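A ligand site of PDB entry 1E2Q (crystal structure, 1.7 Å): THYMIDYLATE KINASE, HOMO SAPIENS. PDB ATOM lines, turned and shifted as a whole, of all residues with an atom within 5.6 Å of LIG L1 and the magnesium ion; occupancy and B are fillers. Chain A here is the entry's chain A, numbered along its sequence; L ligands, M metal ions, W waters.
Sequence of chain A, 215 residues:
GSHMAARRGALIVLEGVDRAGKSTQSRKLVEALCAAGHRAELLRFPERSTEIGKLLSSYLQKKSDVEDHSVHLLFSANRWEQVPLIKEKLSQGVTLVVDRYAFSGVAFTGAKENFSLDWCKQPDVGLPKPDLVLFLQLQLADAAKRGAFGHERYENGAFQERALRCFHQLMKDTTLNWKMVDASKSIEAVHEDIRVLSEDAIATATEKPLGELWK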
ATOM      1  N   VAL A  17      19.683  -0.568 -14.891  1.00  0.00           N
ATOM      2  CA  VAL A  17      20.322   0.478 -14.075  1.00  0.00           C
ATOM      3  C   VAL A  17      20.652  -0.072 -12.709  1.00  0.00           C
ATOM      4  O   VAL A  17      20.280  -1.206 -12.381  1.00  0.00           O
ATOM      5  CB  VAL A  17      19.345   1.672 -13.924  1.00  0.00           C
ATOM      6  CG1 VAL A  17      19.024   2.250 -15.289  1.00  0.00           C
ATOM      7  CG2 VAL A  17      18.102   1.212 -13.175  1.00  0.00           C
ATOM      8  N   ASP A  18      21.315   0.750 -11.876  1.00  0.00           N
ATOM      9  CA  ASP A  18      21.567   0.309 -10.495  1.00  0.00           C
ATOM     10  C   ASP A  18      20.235   0.025  -9.806  1.00  0.00           C
ATOM     11  O   ASP A  18      19.186   0.624 -10.015  1.00  0.00           O
ATOM     12  CB  ASP A  18      22.445   1.380  -9.822  1.00  0.00           C
ATOM     13  CG  ASP A  18      23.820   1.468 -10.432  1.00  0.00           C
ATOM     14  OD1 ASP A  18      24.269   0.414 -10.937  1.00  0.00           O
ATOM     15  OD2 ASP A  18      24.583   2.472 -10.475  1.00  0.00           O
ATOM     16  N   ARG A  19      20.151  -1.043  -9.016  1.00  0.00           N
ATOM     17  CA  ARG A  19      19.033  -1.518  -8.235  1.00  0.00           C
ATOM     18  C   ARG A  19      17.864  -2.163  -8.940  1.00  0.00           C
ATOM     19  O   ARG A  19      16.781  -2.366  -8.378  1.00  0.00           O
ATOM     20  CB  ARG A  19      18.458  -0.441  -7.303  1.00  0.00           C
ATOM     21  CG  ARG A  19      18.960  -0.674  -5.897  1.00  0.00           C
ATOM     22  CD  ARG A  19      19.238   0.570  -5.101  1.00  0.00           C
ATOM     23  NE  ARG A  19      18.277   1.644  -5.323  1.00  0.00           N
ATOM     24  CZ  ARG A  19      18.463   2.820  -4.714  1.00  0.00           C
ATOM     25  NH1 ARG A  19      19.498   3.006  -3.914  1.00  0.00           N
ATOM     26  NH2 ARG A  19      17.599   3.811  -4.906  1.00  0.00           N
ATOM     27  N   ALA A  20      18.046  -2.533 -10.208  1.00  0.00           N
ATOM     28  CA  ALA A  20      17.012  -3.152 -10.997  1.00  0.00           C
ATOM     29  C   ALA A  20      16.747  -4.605 -10.610  1.00  0.00           C
ATOM     30  O   ALA A  20      15.743  -5.160 -11.021  1.00  0.00           O
ATOM     31  CB  ALA A  20      17.418  -3.094 -12.468  1.00  0.00           C
ATOM     32  N   GLY A  21      17.661  -5.198  -9.860  1.00  0.00           N
ATOM     33  CA  GLY A  21      17.528  -6.606  -9.479  1.00  0.00           C
ATOM     34  C   GLY A  21      18.483  -7.517 -10.270  1.00  0.00           C
ATOM     35  O   GLY A  21      18.331  -8.736 -10.262  1.00  0.00           O
ATOM     36  N   LYS A  22      19.473  -6.998 -10.994  1.00  0.00           N
ATOM     37  CA  LYS A  22      20.372  -7.800 -11.780  1.00  0.00           C
ATOM     38  C   LYS A  22      21.096  -8.899 -11.006  1.00  0.00           C
ATOM     39  O   LYS A  22      21.177 -10.049 -11.417  1.00  0.00           O
ATOM     40  CB  LYS A  22      21.485  -6.928 -12.450  1.00  0.00           C
ATOM     41  CG  LYS A  22      20.807  -5.806 -13.265  1.00  0.00           C
ATOM     42  CD  LYS A  22      21.870  -5.023 -14.036  1.00  0.00           C
ATOM     43  CE  LYS A  22      22.829  -4.315 -13.077  1.00  0.00           C
ATOM     44  NZ  LYS A  22      22.090  -3.333 -12.239  1.00  0.00           N
ATOM     45  N   SER A  23      21.671  -8.578  -9.854  1.00  0.00           N
ATOM     46  CA  SER A  23      22.436  -9.541  -9.092  1.00  0.00           C
ATOM     47  C   SER A  23      21.511 -10.603  -8.478  1.00  0.00           C
ATOM     48  O   SER A  23      21.831 -11.798  -8.478  1.00  0.00           O
ATOM     49  CB  SER A  23      23.226  -8.854  -7.976  1.00  0.00           C
ATOM     50  OG  SER A  23      24.193  -8.008  -8.621  1.00  0.00           O
ATOM     51  N   THR A  24      20.369 -10.147  -7.975  1.00  0.00           N
ATOM     52  CA  THR A  24      19.424 -11.100  -7.366  1.00  0.00           C
ATOM     53  C   THR A  24      18.934 -12.077  -8.423  1.00  0.00           C
ATOM     54  O   THR A  24      18.918 -13.309  -8.219  1.00  0.00           O
ATOM     55  CB  THR A  24      18.236 -10.334  -6.777  1.00  0.00           C
ATOM     56  OG1 THR A  24      18.631  -9.537  -5.675  1.00  0.00           O
ATOM     57  CG2 THR A  24      17.200 -11.346  -6.258  1.00  0.00           C
ATOM     58  N   GLN A  25      18.578 -11.523  -9.599  1.00  0.00           N
ATOM     59  CA  GLN A  25      18.059 -12.411 -10.654  1.00  0.00           C
ATOM     60  C   GLN A  25      19.149 -13.266 -11.264  1.00  0.00           C
ATOM     61  O   GLN A  25      18.880 -14.404 -11.655  1.00  0.00           O
ATOM     62  CB  GLN A  25      17.311 -11.568 -11.701  1.00  0.00           C
ATOM     63  CG  GLN A  25      16.029 -10.902 -11.201  1.00  0.00           C
ATOM     64  CD  GLN A  25      15.014 -11.859 -10.607  1.00  0.00           C
ATOM     65  OE1 GLN A  25      14.943 -13.031 -11.005  1.00  0.00           O
ATOM     66  NE2 GLN A  25      14.217 -11.430  -9.644  1.00  0.00           N
ATOM     67  N   ARG A  27      21.774 -14.557  -9.670  1.00  0.00           N
ATOM     68  CA  ARG A  27      21.967 -15.674  -8.730  1.00  0.00           C
ATOM     69  C   ARG A  27      20.818 -16.704  -8.786  1.00  0.00           C
ATOM     70  O   ARG A  27      21.083 -17.926  -8.838  1.00  0.00           O
ATOM     71  CB  ARG A  27      22.022 -15.195  -7.255  1.00  0.00           C
ATOM     72  CG  ARG A  27      23.266 -14.323  -7.000  1.00  0.00           C
ATOM     73  CD  ARG A  27      23.315 -14.060  -5.476  1.00  0.00           C
ATOM     74  NE  ARG A  27      22.197 -13.302  -4.987  1.00  0.00           N
ATOM     75  CZ  ARG A  27      22.116 -11.970  -4.895  1.00  0.00           C
ATOM     76  NH1 ARG A  27      23.132 -11.168  -5.245  1.00  0.00           N
ATOM     77  NH2 ARG A  27      21.012 -11.469  -4.368  1.00  0.00           N
ATOM     78  N   ASP A  99      26.171 -10.943 -14.955  1.00  0.00           N
ATOM     79  CA  ASP A  99      25.598  -9.792 -14.279  1.00  0.00           C
ATOM     80  C   ASP A  99      26.368  -8.538 -14.685  1.00  0.00           C
ATOM     81  O   ASP A  99      27.448  -8.331 -14.119  1.00  0.00           O
ATOM     82  CB  ASP A  99      25.717 -10.111 -12.788  1.00  0.00           C
ATOM     83  CG  ASP A  99      25.155  -9.070 -11.861  1.00  0.00           C
ATOM     84  OD1 ASP A  99      24.610  -8.006 -12.281  1.00  0.00           O
ATOM     85  OD2 ASP A  99      25.355  -9.291 -10.620  1.00  0.00           O
ATOM     86  N   ARG A 100      25.846  -7.837 -15.658  1.00  0.00           N
ATOM     87  CA  ARG A 100      26.385  -6.677 -16.343  1.00  0.00           C
ATOM     88  C   ARG A 100      27.463  -7.109 -17.355  1.00  0.00           C
ATOM     89  O   ARG A 100      28.182  -8.111 -17.151  1.00  0.00           O
ATOM     90  CB  ARG A 100      26.986  -5.587 -15.442  1.00  0.00           C
ATOM     91  CG  ARG A 100      25.955  -4.959 -14.480  1.00  0.00           C
ATOM     92  CD  ARG A 100      26.698  -3.785 -13.806  1.00  0.00           C
ATOM     93  NE  ARG A 100      25.892  -2.939 -12.974  1.00  0.00           N
ATOM     94  CZ  ARG A 100      25.024  -1.970 -13.234  1.00  0.00           C
ATOM     95  NH1 ARG A 100      24.667  -1.549 -14.449  1.00  0.00           N
ATOM     96  NH2 ARG A 100      24.497  -1.476 -12.090  1.00  0.00           N
ATOM     97  N   ARG A 146      14.170   1.267  -3.607  1.00  0.00           N
ATOM     98  CA  ARG A 146      14.638  -0.046  -3.184  1.00  0.00           C
ATOM     99  C   ARG A 146      15.715   0.317  -2.162  1.00  0.00           C
ATOM    100  O   ARG A 146      16.905   0.188  -2.371  1.00  0.00           O
ATOM    101  CB  ARG A 146      15.147  -0.989  -4.263  1.00  0.00           C
ATOM    102  CG  ARG A 146      13.956  -1.773  -4.796  1.00  0.00           C
ATOM    103  CD  ARG A 146      14.231  -2.335  -6.194  1.00  0.00           C
ATOM    104  NE  ARG A 146      12.944  -2.791  -6.717  1.00  0.00           N
ATOM    105  CZ  ARG A 146      12.895  -3.649  -7.745  1.00  0.00           C
ATOM    106  NH1 ARG A 146      14.056  -4.050  -8.260  1.00  0.00           N
ATOM    107  NH2 ARG A 146      11.736  -4.039  -8.194  1.00  0.00           N
ATOM    108  N   GLU A 155      25.972   6.767  -7.952  1.00  0.00           N
ATOM    109  CA  GLU A 155      24.759   6.560  -7.151  1.00  0.00           C
ATOM    110  C   GLU A 155      23.892   7.799  -6.994  1.00  0.00           C
ATOM    111  O   GLU A 155      23.631   8.161  -5.834  1.00  0.00           O
ATOM    112  CB  GLU A 155      25.147   6.042  -5.757  1.00  0.00           C
ATOM    113  CG  GLU A 155      25.853   4.701  -5.737  1.00  0.00           C
ATOM    114  CD  GLU A 155      24.967   3.551  -5.283  1.00  0.00           C
ATOM    115  OE1 GLU A 155      23.956   3.831  -4.596  1.00  0.00           O
ATOM    116  OE2 GLU A 155      25.273   2.374  -5.602  1.00  0.00           O
ATOM    117  N   ALA A 183      10.799  -5.582 -14.276  1.00  0.00           N
ATOM    118  CA  ALA A 183      11.472  -5.810 -13.003  1.00  0.00           C
ATOM    119  C   ALA A 183      10.798  -5.164 -11.808  1.00  0.00           C
ATOM    120  O   ALA A 183      11.357  -5.194 -10.721  1.00  0.00           O
ATOM    121  CB  ALA A 183      12.913  -5.299 -13.129  1.00  0.00           C
ATOM    122  N   SER A 184       9.605  -4.595 -12.026  1.00  0.00           N
ATOM    123  CA  SER A 184       8.853  -4.008 -10.919  1.00  0.00           C
ATOM    124  C   SER A 184       8.062  -5.053 -10.166  1.00  0.00           C
ATOM    125  O   SER A 184       7.556  -4.778  -9.059  1.00  0.00           O
ATOM    126  CB  SER A 184       7.898  -2.920 -11.447  1.00  0.00           C
ATOM    127  OG  SER A 184       6.793  -3.519 -12.108  1.00  0.00           O
ATOM    128  N   LYS A 185       7.942  -6.261 -10.725  1.00  0.00           N
ATOM    129  CA  LYS A 185       7.183  -7.308 -10.027  1.00  0.00           C
ATOM    130  C   LYS A 185       7.962  -7.927  -8.872  1.00  0.00           C
ATOM    131  O   LYS A 185       9.054  -7.447  -8.585  1.00  0.00           O
ATOM    132  CB  LYS A 185       6.747  -8.370 -11.034  1.00  0.00           C
ATOM    133  CG  LYS A 185       5.994  -7.683 -12.187  1.00  0.00           C
ATOM    134  CD  LYS A 185       5.319  -8.712 -13.077  1.00  0.00           C
ATOM    135  CE  LYS A 185       6.280  -9.550 -13.878  1.00  0.00           C
ATOM    136  NZ  LYS A 185       5.573 -10.316 -14.949  1.00  0.00           N
ATOM    137  N   SER A 186       7.400  -8.954  -8.225  1.00  0.00           N
ATOM    138  CA  SER A 186       8.068  -9.547  -7.073  1.00  0.00           C
ATOM    139  C   SER A 186       9.370 -10.253  -7.495  1.00  0.00           C
ATOM    140  O   SER A 186       9.457 -10.582  -8.675  1.00  0.00           O
ATOM    141  CB  SER A 186       7.171 -10.582  -6.426  1.00  0.00           C
ATOM    142  OG  SER A 186       6.973 -11.766  -7.192  1.00  0.00           O
ATOM    143  N   ILE A 187      10.235 -10.572  -6.537  1.00  0.00           N
ATOM    144  CA  ILE A 187      11.448 -11.309  -6.930  1.00  0.00           C
ATOM    145  C   ILE A 187      11.107 -12.618  -7.615  1.00  0.00           C
ATOM    146  O   ILE A 187      11.723 -12.971  -8.640  1.00  0.00           O
ATOM    147  CB  ILE A 187      12.338 -11.517  -5.676  1.00  0.00           C
ATOM    148  CG1 ILE A 187      12.921 -10.159  -5.284  1.00  0.00           C
ATOM    149  CG2 ILE A 187      13.417 -12.559  -5.915  1.00  0.00           C
ATOM    150  CD1 ILE A 187      13.766 -10.301  -4.025  1.00  0.00           C
ATOM    151  N   VAL A 190       9.505 -11.955 -11.252  1.00  0.00           N
ATOM    152  CA  VAL A 190      10.546 -11.552 -12.237  1.00  0.00           C
ATOM    153  C   VAL A 190      11.384 -12.775 -12.585  1.00  0.00           C
ATOM    154  O   VAL A 190      11.770 -12.981 -13.738  1.00  0.00           O
ATOM    155  CB  VAL A 190      11.378 -10.443 -11.590  1.00  0.00           C
ATOM    156  CG1 VAL A 190      12.532  -9.991 -12.506  1.00  0.00           C
ATOM    157  CG2 VAL A 190      10.460  -9.236 -11.344  1.00  0.00           C
HETATM  158  P1  LIG L   1      23.439  -2.826  -8.471  1.00  0.00           P
HETATM  159  O1  LIG L   1      23.755  -1.908  -7.327  1.00  0.00           O
HETATM  160  O2  LIG L   1      23.078  -2.092  -9.692  1.00  0.00           O
HETATM  161  O3  LIG L   1      24.501  -3.881  -8.463  1.00  0.00           O
HETATM  162  P2  LIG L   1      21.238  -4.737  -8.806  1.00  0.00           P
HETATM  163  O4  LIG L   1      22.274  -5.775  -8.814  1.00  0.00           O
HETATM  164  O5  LIG L   1      20.555  -4.449 -10.077  1.00  0.00           O
HETATM  165  O6  LIG L   1      21.971  -3.435  -8.146  1.00  0.00           O
HETATM  166  P3  LIG L   1      20.035  -6.160  -6.540  1.00  0.00           P
HETATM  167  O7  LIG L   1      19.702  -7.482  -7.135  1.00  0.00           O
HETATM  168  O8  LIG L   1      21.225  -6.117  -5.664  1.00  0.00           O
HETATM  169  O9  LIG L   1      20.125  -5.088  -7.733  1.00  0.00           O
HETATM  170  O10 LIG L   1      18.800  -5.650  -5.747  1.00  0.00           O
HETATM  171  C1  LIG L   1      18.868  -4.354  -5.028  1.00  0.00           C
HETATM  172  C2  LIG L   1      17.956  -4.375  -3.929  1.00  0.00           C
HETATM  173  O11 LIG L   1      16.585  -4.495  -4.300  1.00  0.00           O
HETATM  174  C3  LIG L   1      18.259  -5.560  -3.002  1.00  0.00           C
HETATM  175  O12 LIG L   1      18.018  -5.205  -1.612  1.00  0.00           O
HETATM  176  C4  LIG L   1      17.201  -6.583  -3.358  1.00  0.00           C
HETATM  177  O13 LIG L   1      16.760  -7.531  -2.407  1.00  0.00           O
HETATM  178  C5  LIG L   1      15.986  -5.675  -3.703  1.00  0.00           C
HETATM  179  N1  LIG L   1      15.248  -6.263  -4.855  1.00  0.00           N
HETATM  180  C6  LIG L   1      15.748  -7.033  -5.913  1.00  0.00           C
HETATM  181  N2  LIG L   1      14.720  -7.358  -6.668  1.00  0.00           N
HETATM  182  C7  LIG L   1      13.566  -6.854  -6.132  1.00  0.00           C
HETATM  183  C8  LIG L   1      12.214  -6.911  -6.507  1.00  0.00           C
HETATM  184  N3  LIG L   1      11.813  -7.589  -7.586  1.00  0.00           N
HETATM  185  N4  LIG L   1      11.442  -6.252  -5.664  1.00  0.00           N
HETATM  186  C9  LIG L   1      11.817  -5.546  -4.573  1.00  0.00           C
HETATM  187  N5  LIG L   1      13.084  -5.463  -4.183  1.00  0.00           N
HETATM  188  C10 LIG L   1      13.853  -6.124  -4.985  1.00  0.00           C
HETATM  189  P1  LG2 L   2      27.142  -3.009  -9.887  1.00  0.00           P
HETATM  190  O1  LG2 L   2      25.907  -2.164  -9.675  1.00  0.00           O
HETATM  191  O2  LG2 L   2      27.038  -4.176 -10.767  1.00  0.00           O
HETATM  192  O3  LG2 L   2      27.767  -3.253  -8.432  1.00  0.00           O
HETATM  193  O4  LG2 L   2      28.240  -2.077 -10.584  1.00  0.00           O
HETATM  194  C1  LG2 L   2      29.011  -1.029  -9.937  1.00  0.00           C
HETATM  195  C2  LG2 L   2      29.110   0.045 -11.054  1.00  0.00           C
HETATM  196  O5  LG2 L   2      29.947  -0.101 -12.180  1.00  0.00           O
HETATM  197  C3  LG2 L   2      27.710   0.383 -11.530  1.00  0.00           C
HETATM  198  O6  LG2 L   2      27.397   1.746 -11.221  1.00  0.00           O
HETATM  199  C4  LG2 L   2      27.812   0.224 -13.055  1.00  0.00           C
HETATM  200  C5  LG2 L   2      29.315   0.416 -13.318  1.00  0.00           C
HETATM  201  N1  LG2 L   2      29.964  -0.099 -14.511  1.00  0.00           N
HETATM  202  C6  LG2 L   2      30.665   0.819 -15.338  1.00  0.00           C
HETATM  203  O7  LG2 L   2      30.697   2.038 -15.159  1.00  0.00           O
HETATM  204  N2  LG2 L   2      31.243   0.219 -16.411  1.00  0.00           N
HETATM  205  C7  LG2 L   2      31.223  -1.145 -16.638  1.00  0.00           C
HETATM  206  O8  LG2 L   2      31.861  -1.642 -17.740  1.00  0.00           O
HETATM  207  C8  LG2 L   2      30.510  -2.052 -15.713  1.00  0.00           C
HETATM  208  C9  LG2 L   2      30.493  -3.528 -16.000  1.00  0.00           C
HETATM  209  C10 LG2 L   2      29.913  -1.431 -14.651  1.00  0.00           C
HETATM  210 MG    MG M   1      24.304  -5.912  -8.485  1.00  0.00          MG
HETATM  211  O   HOH W   1       8.642  -5.611  -6.318  1.00  0.00           O
HETATM  212  O   HOH W   2      24.822  -5.971 -10.617  1.00  0.00           O
HETATM  213  O   HOH W   3      18.269  -9.465  -2.982  1.00  0.00           O
HETATM  214  O   HOH W   4      23.849  -6.012  -6.438  1.00  0.00           O
HETATM  215  O   HOH W   5      13.392  -3.809  -1.827  1.00  0.00           O
HETATM  216  O   HOH W   6      26.312  -6.161  -7.972  1.00  0.00           O
HETATM  217  O   HOH W   7      20.310  -4.134  -1.067  1.00  0.00           O
HETATM  218  O   HOH W   8      22.088  -5.292  -3.209  1.00  0.00           O
HETATM  219  O   HOH W   9      14.218  -8.678  -9.125  1.00  0.00           O
HETATM  220  O   HOH W  10      14.144  -7.679  -1.165  1.00  0.00           O
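A nitrogen (N4) of LIG L1 sits close to the guanidinium group of Arg 146 (3.4 Å).
The guanidinium group (NE) of Arg 100 lies within salt-bridge range of an oxygen (O2) of LG2 L2 (2.8 Å).
N of Lys 22 lies within hydrogen-bond range of O5 of LIG L1 (2.9 Å).
The backbone NH (N) of Ala 20 sits at hydrogen-bond distance from an oxygen (O5) of LIG L1, 3.2 Å away.
N3 of LIG L1 is in hydrogen-bond range of O of Lys 185 (2.9 Å).
An oxygen (O2) of LIG L1 lies within salt-bridge range of the guanidinium group (NH2) of Arg 100 (2.9 Å).
An oxygen (O7) of LIG L1 lies within hydrogen-bond range of the side-chain hydroxyl (OG1) of Thr 24 (2.7 Å).
The backbone NH of Thr 24 sits at hydrogen-bond distance from an oxygen (O7) of LIG L1 (2.9 Å).
The side-chain carboxylate (OD1) of Asp 18 lies close to an oxygen (O2) of LIG L1.
An oxygen (O6) of LIG L1 is in hydrogen-bond range of the backbone NH (N) of Arg 19.
An oxygen (O5) of LIG L1 is in hydrogen-bond range of the backbone NH of Gly 21, at 3.0 Å.
The side-chain amino group (NZ) of Lys 22 is in salt-bridge range of an oxygen (O5) of LIG L1 (2.9 Å).
O4 of LIG L1 lies close to N of Ser 23, 3.0 Å away.
The side-chain carboxylate (OD2) of Asp 18 is in hydrogen-bond range of an oxygen (O6) of LG2 L2, 3.0 Å away.
An oxygen (O3) of LIG L1 sits close to an oxygen (O1) of LG2 L2.
The backbone carbonyl oxygen (O) of Ala 183 is in hydrogen-bond range of the guanidinium group (NH2) of Arg 146 (2.8 Å).
The backbone carbonyl oxygen of Ile 187 is in hydrogen-bond range of the side-chain amide nitrogen of Gln 25, at 3.1 Å.
The guanidinium group (NH2) of Arg 27 is in hydrogen-bond range of the side-chain hydroxyl (OG1) of Thr 24 (3.3 Å).
NZ of Lys 22 lies within hydrogen-bond range of O of Val 17, 2.8 Å away.
The backbone carbonyl oxygen (O) of Ala 20 is in hydrogen-bond range of the guanidinium group (NH1) of Arg 146 (3.4 Å).
The side-chain carboxylate of Asp 99 sits close to the side-chain hydroxyl of Ser 23, at 2.6 Å.
O of Arg 19 lies within hydrogen-bond range of NH1 of Arg 146 (3.2 Å).
Residues that only touch LIG L1: Ile 187, Ser 186, Ala 183 and Val 17.
The nearest printed residue that does not touch LIG L1 is Val 190 (4.3 Å).
One residue has an atom within 4 Å of the magnesium ion: Ser 23.
The nearest printed residue that does not touch the magnesium ion is Asp 99 (4.1 Å).
The magnesium ion is bound by an oxygen (O3) of LIG L1 (2.0 Å), an oxygen (O4) of LIG L1 (2.1 Å), water W6 (2.1 Å), water W4 (2.1 Å), the side-chain hydroxyl of Ser 23 (2.1 Å) and water W2 (2.2 Å).
Water W2 bridges the side-chain carboxylate (OD1) of Asp 99 (2.6 Å) and an oxygen (O2) of LG2 L2 (2.9 Å).
Water W3 bridges O13 of LIG L1 (2.5 Å) and OG1 of Thr 24 (2.7 Å).
Water W9 bridges the side-chain amide nitrogen (NE2) of Gln 25 and a nitrogen (N2) of LIG L1.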
